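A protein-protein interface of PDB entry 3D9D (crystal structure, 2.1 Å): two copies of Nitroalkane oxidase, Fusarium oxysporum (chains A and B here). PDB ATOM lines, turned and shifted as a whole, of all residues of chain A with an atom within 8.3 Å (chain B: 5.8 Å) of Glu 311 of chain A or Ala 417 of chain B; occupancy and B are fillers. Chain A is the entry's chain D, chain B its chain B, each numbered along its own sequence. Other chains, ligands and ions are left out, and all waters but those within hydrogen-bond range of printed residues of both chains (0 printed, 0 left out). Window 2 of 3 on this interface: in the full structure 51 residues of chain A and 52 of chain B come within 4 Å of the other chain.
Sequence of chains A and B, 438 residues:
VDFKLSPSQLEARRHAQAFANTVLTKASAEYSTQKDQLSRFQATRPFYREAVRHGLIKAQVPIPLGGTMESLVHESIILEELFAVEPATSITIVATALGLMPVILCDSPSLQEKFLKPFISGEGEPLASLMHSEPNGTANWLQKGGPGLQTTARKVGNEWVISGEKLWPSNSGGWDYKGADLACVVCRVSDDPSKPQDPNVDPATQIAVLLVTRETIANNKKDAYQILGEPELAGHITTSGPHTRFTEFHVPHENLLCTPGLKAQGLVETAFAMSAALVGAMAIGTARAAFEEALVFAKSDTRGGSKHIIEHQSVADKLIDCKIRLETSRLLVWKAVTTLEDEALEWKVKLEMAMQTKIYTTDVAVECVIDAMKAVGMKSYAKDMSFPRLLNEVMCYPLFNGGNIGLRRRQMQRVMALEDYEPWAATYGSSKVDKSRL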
ATOM      1  N   LEU A 295      20.440   1.191  -1.230  1.00  0.00           N
ATOM      2  CA  LEU A 295      20.023   2.370  -1.943  1.00  0.00           C
ATOM      3  C   LEU A 295      21.233   3.179  -2.442  1.00  0.00           C
ATOM      4  O   LEU A 295      21.312   3.563  -3.627  1.00  0.00           O
ATOM      5  CB  LEU A 295      19.139   3.242  -1.042  1.00  0.00           C
ATOM      6  CG  LEU A 295      18.712   4.585  -1.641  1.00  0.00           C
ATOM      7  CD1 LEU A 295      17.698   4.382  -2.807  1.00  0.00           C
ATOM      8  CD2 LEU A 295      18.122   5.494  -0.536  1.00  0.00           C
ATOM      9  N   ALA A 298      22.914   1.335  -5.262  1.00  0.00           N
ATOM     10  CA  ALA A 298      22.188   1.262  -6.524  1.00  0.00           C
ATOM     11  C   ALA A 298      22.203   2.588  -7.269  1.00  0.00           C
ATOM     12  O   ALA A 298      21.959   2.633  -8.504  1.00  0.00           O
ATOM     13  CB  ALA A 298      20.776   0.800  -6.318  1.00  0.00           C
ATOM     14  N   LYS A 299      22.504   3.652  -6.531  1.00  0.00           N
ATOM     15  CA  LYS A 299      22.549   5.006  -7.083  1.00  0.00           C
ATOM     16  C   LYS A 299      23.953   5.415  -7.448  1.00  0.00           C
ATOM     17  O   LYS A 299      24.154   6.467  -8.037  1.00  0.00           O
ATOM     18  CB  LYS A 299      21.984   6.014  -6.075  1.00  0.00           C
ATOM     19  CG  LYS A 299      20.461   6.011  -5.979  1.00  0.00           C
ATOM     20  CD  LYS A 299      20.019   6.728  -4.696  1.00  0.00           C
ATOM     21  CE  LYS A 299      20.159   8.241  -4.846  1.00  0.00           C
ATOM     22  NZ  LYS A 299      18.851   8.894  -4.858  1.00  0.00           N
ATOM     23  N   SER A 300      24.927   4.579  -7.103  1.00  0.00           N
ATOM     24  CA  SER A 300      26.328   4.886  -7.329  1.00  0.00           C
ATOM     25  C   SER A 300      27.017   3.871  -8.212  1.00  0.00           C
ATOM     26  O   SER A 300      28.182   4.075  -8.568  1.00  0.00           O
ATOM     27  CB  SER A 300      27.089   4.830  -5.995  1.00  0.00           C
ATOM     28  OG  SER A 300      26.480   5.690  -5.077  1.00  0.00           O
ATOM     29  N   ASP A 301      26.377   2.741  -8.488  1.00  0.00           N
ATOM     30  CA  ASP A 301      27.110   1.667  -9.137  1.00  0.00           C
ATOM     31  C   ASP A 301      26.323   1.171 -10.347  1.00  0.00           C
ATOM     32  O   ASP A 301      25.073   1.065 -10.287  1.00  0.00           O
ATOM     33  CB  ASP A 301      27.382   0.552  -8.128  1.00  0.00           C
ATOM     34  CG  ASP A 301      28.434  -0.432  -8.597  1.00  0.00           C
ATOM     35  OD1 ASP A 301      28.121  -1.260  -9.492  1.00  0.00           O
ATOM     36  OD2 ASP A 301      29.563  -0.420  -8.029  1.00  0.00           O
ATOM     37  N   SER A 306      25.850   0.677 -18.325  1.00  0.00           N
ATOM     38  CA  SER A 306      25.980   2.097 -18.640  1.00  0.00           C
ATOM     39  C   SER A 306      25.239   2.993 -17.629  1.00  0.00           C
ATOM     40  O   SER A 306      25.584   4.173 -17.476  1.00  0.00           O
ATOM     41  CB  SER A 306      25.536   2.390 -20.076  1.00  0.00           C
ATOM     42  OG  SER A 306      24.178   2.025 -20.237  1.00  0.00           O
ATOM     43  N   LYS A 307      24.235   2.440 -16.947  1.00  0.00           N
ATOM     44  CA  LYS A 307      23.465   3.209 -15.961  1.00  0.00           C
ATOM     45  C   LYS A 307      23.492   2.634 -14.548  1.00  0.00           C
ATOM     46  O   LYS A 307      23.693   1.428 -14.349  1.00  0.00           O
ATOM     47  CB  LYS A 307      21.999   3.492 -16.398  1.00  0.00           C
ATOM     48  CG  LYS A 307      21.409   2.608 -17.473  1.00  0.00           C
ATOM     49  CD  LYS A 307      19.869   2.815 -17.613  1.00  0.00           C
ATOM     50  CE  LYS A 307      19.149   1.448 -17.857  1.00  0.00           C
ATOM     51  NZ  LYS A 307      17.637   1.471 -18.134  1.00  0.00           N
ATOM     52  N   HIS A 308      23.329   3.529 -13.574  1.00  0.00           N
ATOM     53  CA  HIS A 308      23.246   3.159 -12.183  1.00  0.00           C
ATOM     54  C   HIS A 308      22.128   2.104 -12.110  1.00  0.00           C
ATOM     55  O   HIS A 308      21.097   2.224 -12.812  1.00  0.00           O
ATOM     56  CB  HIS A 308      22.939   4.399 -11.317  1.00  0.00           C
ATOM     57  CG  HIS A 308      24.062   5.392 -11.272  1.00  0.00           C
ATOM     58  ND1 HIS A 308      25.384   5.021 -11.104  1.00  0.00           N
ATOM     59  CD2 HIS A 308      24.061   6.744 -11.338  1.00  0.00           C
ATOM     60  CE1 HIS A 308      26.143   6.100 -11.078  1.00  0.00           C
ATOM     61  NE2 HIS A 308      25.368   7.158 -11.222  1.00  0.00           N
ATOM     62  N   ILE A 309      22.361   1.048 -11.327  1.00  0.00           N
ATOM     63  CA  ILE A 309      21.420  -0.096 -11.312  1.00  0.00           C
ATOM     64  C   ILE A 309      20.014   0.266 -10.813  1.00  0.00           C
ATOM     65  O   ILE A 309      19.030  -0.425 -11.131  1.00  0.00           O
ATOM     66  CB  ILE A 309      22.007  -1.364 -10.619  1.00  0.00           C
ATOM     67  CG1 ILE A 309      22.190  -1.152  -9.095  1.00  0.00           C
ATOM     68  CG2 ILE A 309      23.344  -1.768 -11.290  1.00  0.00           C
ATOM     69  CD1 ILE A 309      22.633  -2.426  -8.322  1.00  0.00           C
ATOM     70  N   ILE A 310      19.898   1.386 -10.096  1.00  0.00           N
ATOM     71  CA  ILE A 310      18.554   1.903  -9.713  1.00  0.00           C
ATOM     72  C   ILE A 310      17.644   2.203 -10.897  1.00  0.00           C
ATOM     73  O   ILE A 310      16.422   2.265 -10.751  1.00  0.00           O
ATOM     74  CB  ILE A 310      18.639   3.144  -8.797  1.00  0.00           C
ATOM     75  CG1 ILE A 310      17.276   3.425  -8.151  1.00  0.00           C
ATOM     76  CG2 ILE A 310      19.206   4.363  -9.571  1.00  0.00           C
ATOM     77  CD1 ILE A 310      17.356   3.903  -6.749  1.00  0.00           C
ATOM     78  N   GLU A 311      18.222   2.327 -12.085  1.00  0.00           N
ATOM     79  CA  GLU A 311      17.430   2.554 -13.275  1.00  0.00           C
ATOM     80  C   GLU A 311      16.758   1.268 -13.798  1.00  0.00           C
ATOM     81  O   GLU A 311      15.815   1.327 -14.606  1.00  0.00           O
ATOM     82  CB  GLU A 311      18.305   3.171 -14.356  1.00  0.00           C
ATOM     83  CG  GLU A 311      17.729   4.466 -14.879  1.00  0.00           C
ATOM     84  CD  GLU A 311      18.085   5.650 -14.015  1.00  0.00           C
ATOM     85  OE1 GLU A 311      19.293   5.970 -13.939  1.00  0.00           O
ATOM     86  OE2 GLU A 311      17.168   6.270 -13.431  1.00  0.00           O
ATOM     87  N   HIS A 312      17.241   0.113 -13.347  1.00  0.00           N
ATOM     88  CA  HIS A 312      16.639  -1.158 -13.734  1.00  0.00           C
ATOM     89  C   HIS A 312      15.381  -1.362 -12.907  1.00  0.00           C
ATOM     90  O   HIS A 312      15.445  -1.318 -11.670  1.00  0.00           O
ATOM     91  CB  HIS A 312      17.642  -2.317 -13.531  1.00  0.00           C
ATOM     92  CG  HIS A 312      18.898  -2.161 -14.339  1.00  0.00           C
ATOM     93  ND1 HIS A 312      18.876  -1.955 -15.698  1.00  0.00           N
ATOM     94  CD2 HIS A 312      20.203  -2.166 -13.986  1.00  0.00           C
ATOM     95  CE1 HIS A 312      20.109  -1.817 -16.153  1.00  0.00           C
ATOM     96  NE2 HIS A 312      20.936  -1.950 -15.135  1.00  0.00           N
ATOM     97  N   GLN A 313      14.247  -1.578 -13.566  1.00  0.00           N
ATOM     98  CA  GLN A 313      12.987  -1.693 -12.838  1.00  0.00           C
ATOM     99  C   GLN A 313      12.964  -2.795 -11.796  1.00  0.00           C
ATOM    100  O   GLN A 313      12.368  -2.600 -10.737  1.00  0.00           O
ATOM    101  CB  GLN A 313      11.781  -1.842 -13.753  1.00  0.00           C
ATOM    102  CG  GLN A 313      11.582  -0.712 -14.708  1.00  0.00           C
ATOM    103  CD  GLN A 313      10.343  -0.920 -15.561  1.00  0.00           C
ATOM    104  OE1 GLN A 313       9.826  -2.032 -15.663  1.00  0.00           O
ATOM    105  NE2 GLN A 313       9.886   0.146 -16.218  1.00  0.00           N
ATOM    106  N   SER A 314      13.598  -3.940 -12.071  1.00  0.00           N
ATOM    107  CA  SER A 314      13.638  -5.017 -11.067  1.00  0.00           C
ATOM    108  C   SER A 314      14.375  -4.593  -9.796  1.00  0.00           C
ATOM    109  O   SER A 314      13.991  -4.976  -8.693  1.00  0.00           O
ATOM    110  CB  SER A 314      14.273  -6.286 -11.631  1.00  0.00           C
ATOM    111  OG  SER A 314      13.403  -6.839 -12.572  1.00  0.00           O
ATOM    112  N   VAL A 315      15.430  -3.810  -9.955  1.00  0.00           N
ATOM    113  CA  VAL A 315      16.239  -3.378  -8.838  1.00  0.00           C
ATOM    114  C   VAL A 315      15.430  -2.370  -8.014  1.00  0.00           C
ATOM    115  O   VAL A 315      15.368  -2.452  -6.775  1.00  0.00           O
ATOM    116  CB  VAL A 315      17.547  -2.744  -9.337  1.00  0.00           C
ATOM    117  CG1 VAL A 315      18.309  -2.015  -8.192  1.00  0.00           C
ATOM    118  CG2 VAL A 315      18.426  -3.812 -10.012  1.00  0.00           C
ATOM    119  N   ALA A 316      14.794  -1.448  -8.728  1.00  0.00           N
ATOM    120  CA  ALA A 316      13.961  -0.430  -8.127  1.00  0.00           C
ATOM    121  C   ALA A 316      12.757  -1.045  -7.407  1.00  0.00           C
ATOM    122  O   ALA A 316      12.406  -0.597  -6.332  1.00  0.00           O
ATOM    123  CB  ALA A 316      13.491   0.582  -9.191  1.00  0.00           C
ATOM    124  N   ASP A 317      12.112  -2.035  -8.023  1.00  0.00           N
ATOM    125  CA  ASP A 317      11.060  -2.825  -7.363  1.00  0.00           C
ATOM    126  C   ASP A 317      11.438  -3.365  -5.982  1.00  0.00           C
ATOM    127  O   ASP A 317      10.654  -3.246  -5.041  1.00  0.00           O
ATOM    128  CB  ASP A 317      10.583  -3.947  -8.294  1.00  0.00           C
ATOM    129  CG  ASP A 317       9.650  -3.423  -9.419  1.00  0.00           C
ATOM    130  OD1 ASP A 317       9.378  -4.197 -10.355  1.00  0.00           O
ATOM    131  OD2 ASP A 317       9.180  -2.240  -9.359  1.00  0.00           O
ATOM    132  N   LEU A 319      13.848  -2.114  -3.993  1.00  0.00           N
ATOM    133  CA  LEU A 319      14.111  -0.973  -3.091  1.00  0.00           C
ATOM    134  C   LEU A 319      12.801  -0.363  -2.671  1.00  0.00           C
ATOM    135  O   LEU A 319      12.653   0.035  -1.545  1.00  0.00           O
ATOM    136  CB  LEU A 319      15.007   0.088  -3.739  1.00  0.00           C
ATOM    137  CG  LEU A 319      16.443  -0.381  -3.979  1.00  0.00           C
ATOM    138  CD1 LEU A 319      17.211   0.628  -4.854  1.00  0.00           C
ATOM    139  CD2 LEU A 319      17.182  -0.667  -2.664  1.00  0.00           C
ATOM    140  N   MET B 412       7.604   6.491  -8.428  1.00  0.00           N
ATOM    141  CA  MET B 412       8.372   6.379  -7.213  1.00  0.00           C
ATOM    142  C   MET B 412       9.840   6.128  -7.525  1.00  0.00           C
ATOM    143  O   MET B 412      10.722   6.744  -6.937  1.00  0.00           O
ATOM    144  CB  MET B 412       7.788   5.285  -6.310  1.00  0.00           C
ATOM    145  CG  MET B 412       8.510   5.210  -4.964  1.00  0.00           C
ATOM    146  SD  MET B 412       7.680   4.122  -3.771  1.00  0.00           S
ATOM    147  CE  MET B 412       8.898   4.135  -2.448  1.00  0.00           C
ATOM    148  N   GLN B 413      10.106   5.211  -8.443  1.00  0.00           N
ATOM    149  CA  GLN B 413      11.470   4.933  -8.905  1.00  0.00           C
ATOM    150  C   GLN B 413      12.221   6.234  -9.334  1.00  0.00           C
ATOM    151  O   GLN B 413      13.373   6.468  -8.926  1.00  0.00           O
ATOM    152  CB  GLN B 413      11.407   3.909 -10.060  1.00  0.00           C
ATOM    153  CG  GLN B 413      12.731   3.561 -10.665  1.00  0.00           C
ATOM    154  CD  GLN B 413      12.621   2.578 -11.809  1.00  0.00           C
ATOM    155  OE1 GLN B 413      11.513   2.143 -12.205  1.00  0.00           O
ATOM    156  NE2 GLN B 413      13.772   2.200 -12.349  1.00  0.00           N
ATOM    157  N   ARG B 414      11.561   7.072 -10.132  1.00  0.00           N
ATOM    158  CA  ARG B 414      12.191   8.307 -10.631  1.00  0.00           C
ATOM    159  C   ARG B 414      12.582   9.241  -9.468  1.00  0.00           C
ATOM    160  O   ARG B 414      13.691   9.791  -9.457  1.00  0.00           O
ATOM    161  CB  ARG B 414      11.290   9.015 -11.635  1.00  0.00           C
ATOM    162  N   VAL B 415      11.716   9.347  -8.465  1.00  0.00           N
ATOM    163  CA  VAL B 415      12.023  10.155  -7.273  1.00  0.00           C
ATOM    164  C   VAL B 415      13.201   9.580  -6.518  1.00  0.00           C
ATOM    165  O   VAL B 415      14.139  10.310  -6.157  1.00  0.00           O
ATOM    166  CB  VAL B 415      10.804  10.271  -6.305  1.00  0.00           C
ATOM    167  CG1 VAL B 415      11.239  10.795  -4.921  1.00  0.00           C
ATOM    168  CG2 VAL B 415       9.760  11.182  -6.890  1.00  0.00           C
ATOM    169  N   MET B 416      13.177   8.265  -6.290  1.00  0.00           N
ATOM    170  CA  MET B 416      14.236   7.623  -5.535  1.00  0.00           C
ATOM    171  C   MET B 416      15.587   7.809  -6.209  1.00  0.00           C
ATOM    172  O   MET B 416      16.628   7.880  -5.515  1.00  0.00           O
ATOM    173  CB  MET B 416      13.936   6.138  -5.311  1.00  0.00           C
ATOM    174  CG  MET B 416      12.680   5.853  -4.449  1.00  0.00           C
ATOM    175  SD  MET B 416      12.385   4.062  -4.386  1.00  0.00           S
ATOM    176  CE  MET B 416      13.356   3.600  -2.970  1.00  0.00           C
ATOM    177  N   ALA B 417      15.576   7.891  -7.546  1.00  0.00           N
ATOM    178  CA  ALA B 417      16.811   8.054  -8.312  1.00  0.00           C
ATOM    179  C   ALA B 417      17.421   9.476  -8.291  1.00  0.00           C
ATOM    180  O   ALA B 417      18.602   9.645  -8.597  1.00  0.00           O
ATOM    181  CB  ALA B 417      16.624   7.557  -9.755  1.00  0.00           C
ATOM    182  N   LEU B 418      16.620  10.484  -7.946  1.00  0.00           N
ATOM    183  CA  LEU B 418      17.110  11.861  -7.793  1.00  0.00           C
ATOM    184  C   LEU B 418      18.318  11.973  -6.874  1.00  0.00           C
ATOM    185  O   LEU B 418      18.368  11.363  -5.791  1.00  0.00           O
ATOM    186  CB  LEU B 418      16.002  12.786  -7.308  1.00  0.00           C
ATOM    187  CG  LEU B 418      14.786  12.890  -8.244  1.00  0.00           C
ATOM    188  CD1 LEU B 418      13.795  13.853  -7.665  1.00  0.00           C
ATOM    189  CD2 LEU B 418      15.161  13.289  -9.682  1.00  0.00           C
ATOM    190  N   GLU B 419      19.302  12.748  -7.316  1.00  0.00           N
ATOM    191  CA  GLU B 419      20.507  12.988  -6.525  1.00  0.00           C
ATOM    192  C   GLU B 419      20.247  13.488  -5.087  1.00  0.00           C
ATOM    193  O   GLU B 419      21.032  13.201  -4.179  1.00  0.00           O
ATOM    194  CB  GLU B 419      21.452  13.940  -7.278  1.00  0.00           C
ATOM    195  CG  GLU B 419      22.790  13.285  -7.634  1.00  0.00           C
ATOM    196  CD  GLU B 419      23.482  13.943  -8.844  1.00  0.00           C
ATOM    197  OE1 GLU B 419      24.560  14.575  -8.640  1.00  0.00           O
ATOM    198  OE2 GLU B 419      22.944  13.812  -9.990  1.00  0.00           O
ATOM    199  N   TYR B 421      17.368  12.842  -3.304  1.00  0.00           N
ATOM    200  CA  TYR B 421      16.319  12.046  -2.663  1.00  0.00           C
ATOM    201  C   TYR B 421      16.630  11.959  -1.163  1.00  0.00           C
ATOM    202  O   TYR B 421      17.753  11.653  -0.797  1.00  0.00           O
ATOM    203  CB  TYR B 421      16.277  10.645  -3.303  1.00  0.00           C
ATOM    204  CG  TYR B 421      15.338   9.629  -2.638  1.00  0.00           C
ATOM    205  CD1 TYR B 421      15.823   8.409  -2.205  1.00  0.00           C
ATOM    206  CD2 TYR B 421      13.963   9.906  -2.442  1.00  0.00           C
ATOM    207  CE1 TYR B 421      14.970   7.450  -1.609  1.00  0.00           C
ATOM    208  CE2 TYR B 421      13.129   8.969  -1.832  1.00  0.00           C
ATOM    209  CZ  TYR B 421      13.651   7.742  -1.435  1.00  0.00           C
ATOM    210  OH  TYR B 421      12.859   6.800  -0.834  1.00  0.00           O
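The backbone carbonyl oxygen (O) of Ile 310 of chain A lies within hydrogen-bond range of the side-chain amide nitrogen (NE2) of Gln 413 of chain B (3.1 Å). NZ of Lys 299 of chain A sits at hydrogen-bond distance from O of Met 416 of chain B (2.5 Å). O of Leu 418 of chain B is in hydrogen-bond range of NZ of Lys 299 of chain A (2.7 Å). O of Glu 311 of chain A lies within hydrogen-bond range of NE2 of Gln 413 of chain B (3.2 Å).
The backbone carbonyl oxygen of Lys 299 of chain A sits close to a ring nitrogen (NE2) of His 308 of chain A (3.5 Å). N of Ile 310 of chain A is in hydrogen-bond range of O of Ala 298 of chain A (2.9 Å).
Among the printed residues, pairs that only touch across the chains: Ala 316 of chain A with Gln 413 of chain B (3.4 Å), Lys 299 of chain A with Tyr 421 of chain B (3.5 Å), Lys 299 of chain A with Ala 417 of chain B (3.8 Å), Gln 313 of chain A with Gln 413 of chain B (3.8 Å), Leu 295 of chain A with Tyr 421 of chain B (3.9 Å), Leu 319 of chain A with Met 416 of chain B (3.9 Å), Glu 311 of chain A with Ala 417 of chain B (3.9 Å) and His 312 of chain A with Gln 413 of chain B (3.9 Å).
Printed residues of chain B within 4 Å of Lys 299 of chain A: Met 416 (2.5 Å), Ala 417 (3.8 Å), Leu 418 (2.7 Å) and Tyr 421 (3.5 Å). Glu 311 of chain A touches two residues of chain B. Of the printed residues of chain B, Gln 313 of chain A touches Gln 413 (3.8 Å). Ala 417 of chain B touches two residues of chain A. The nearest printed residue of chain B that does not touch Leu 295 of chain A is Met 416 of chain B (4.4 Å).
Of the 18 printed residues of chain A, 8 touch a printed residue of chain B. Among the printed residues, 12 pairs touch across the chains. Among the printed residues, no Asp or Glu carboxylate lies within 4 Å of a Lys or Arg side-chain nitrogen of the other chain.
No position is printed for both chains.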
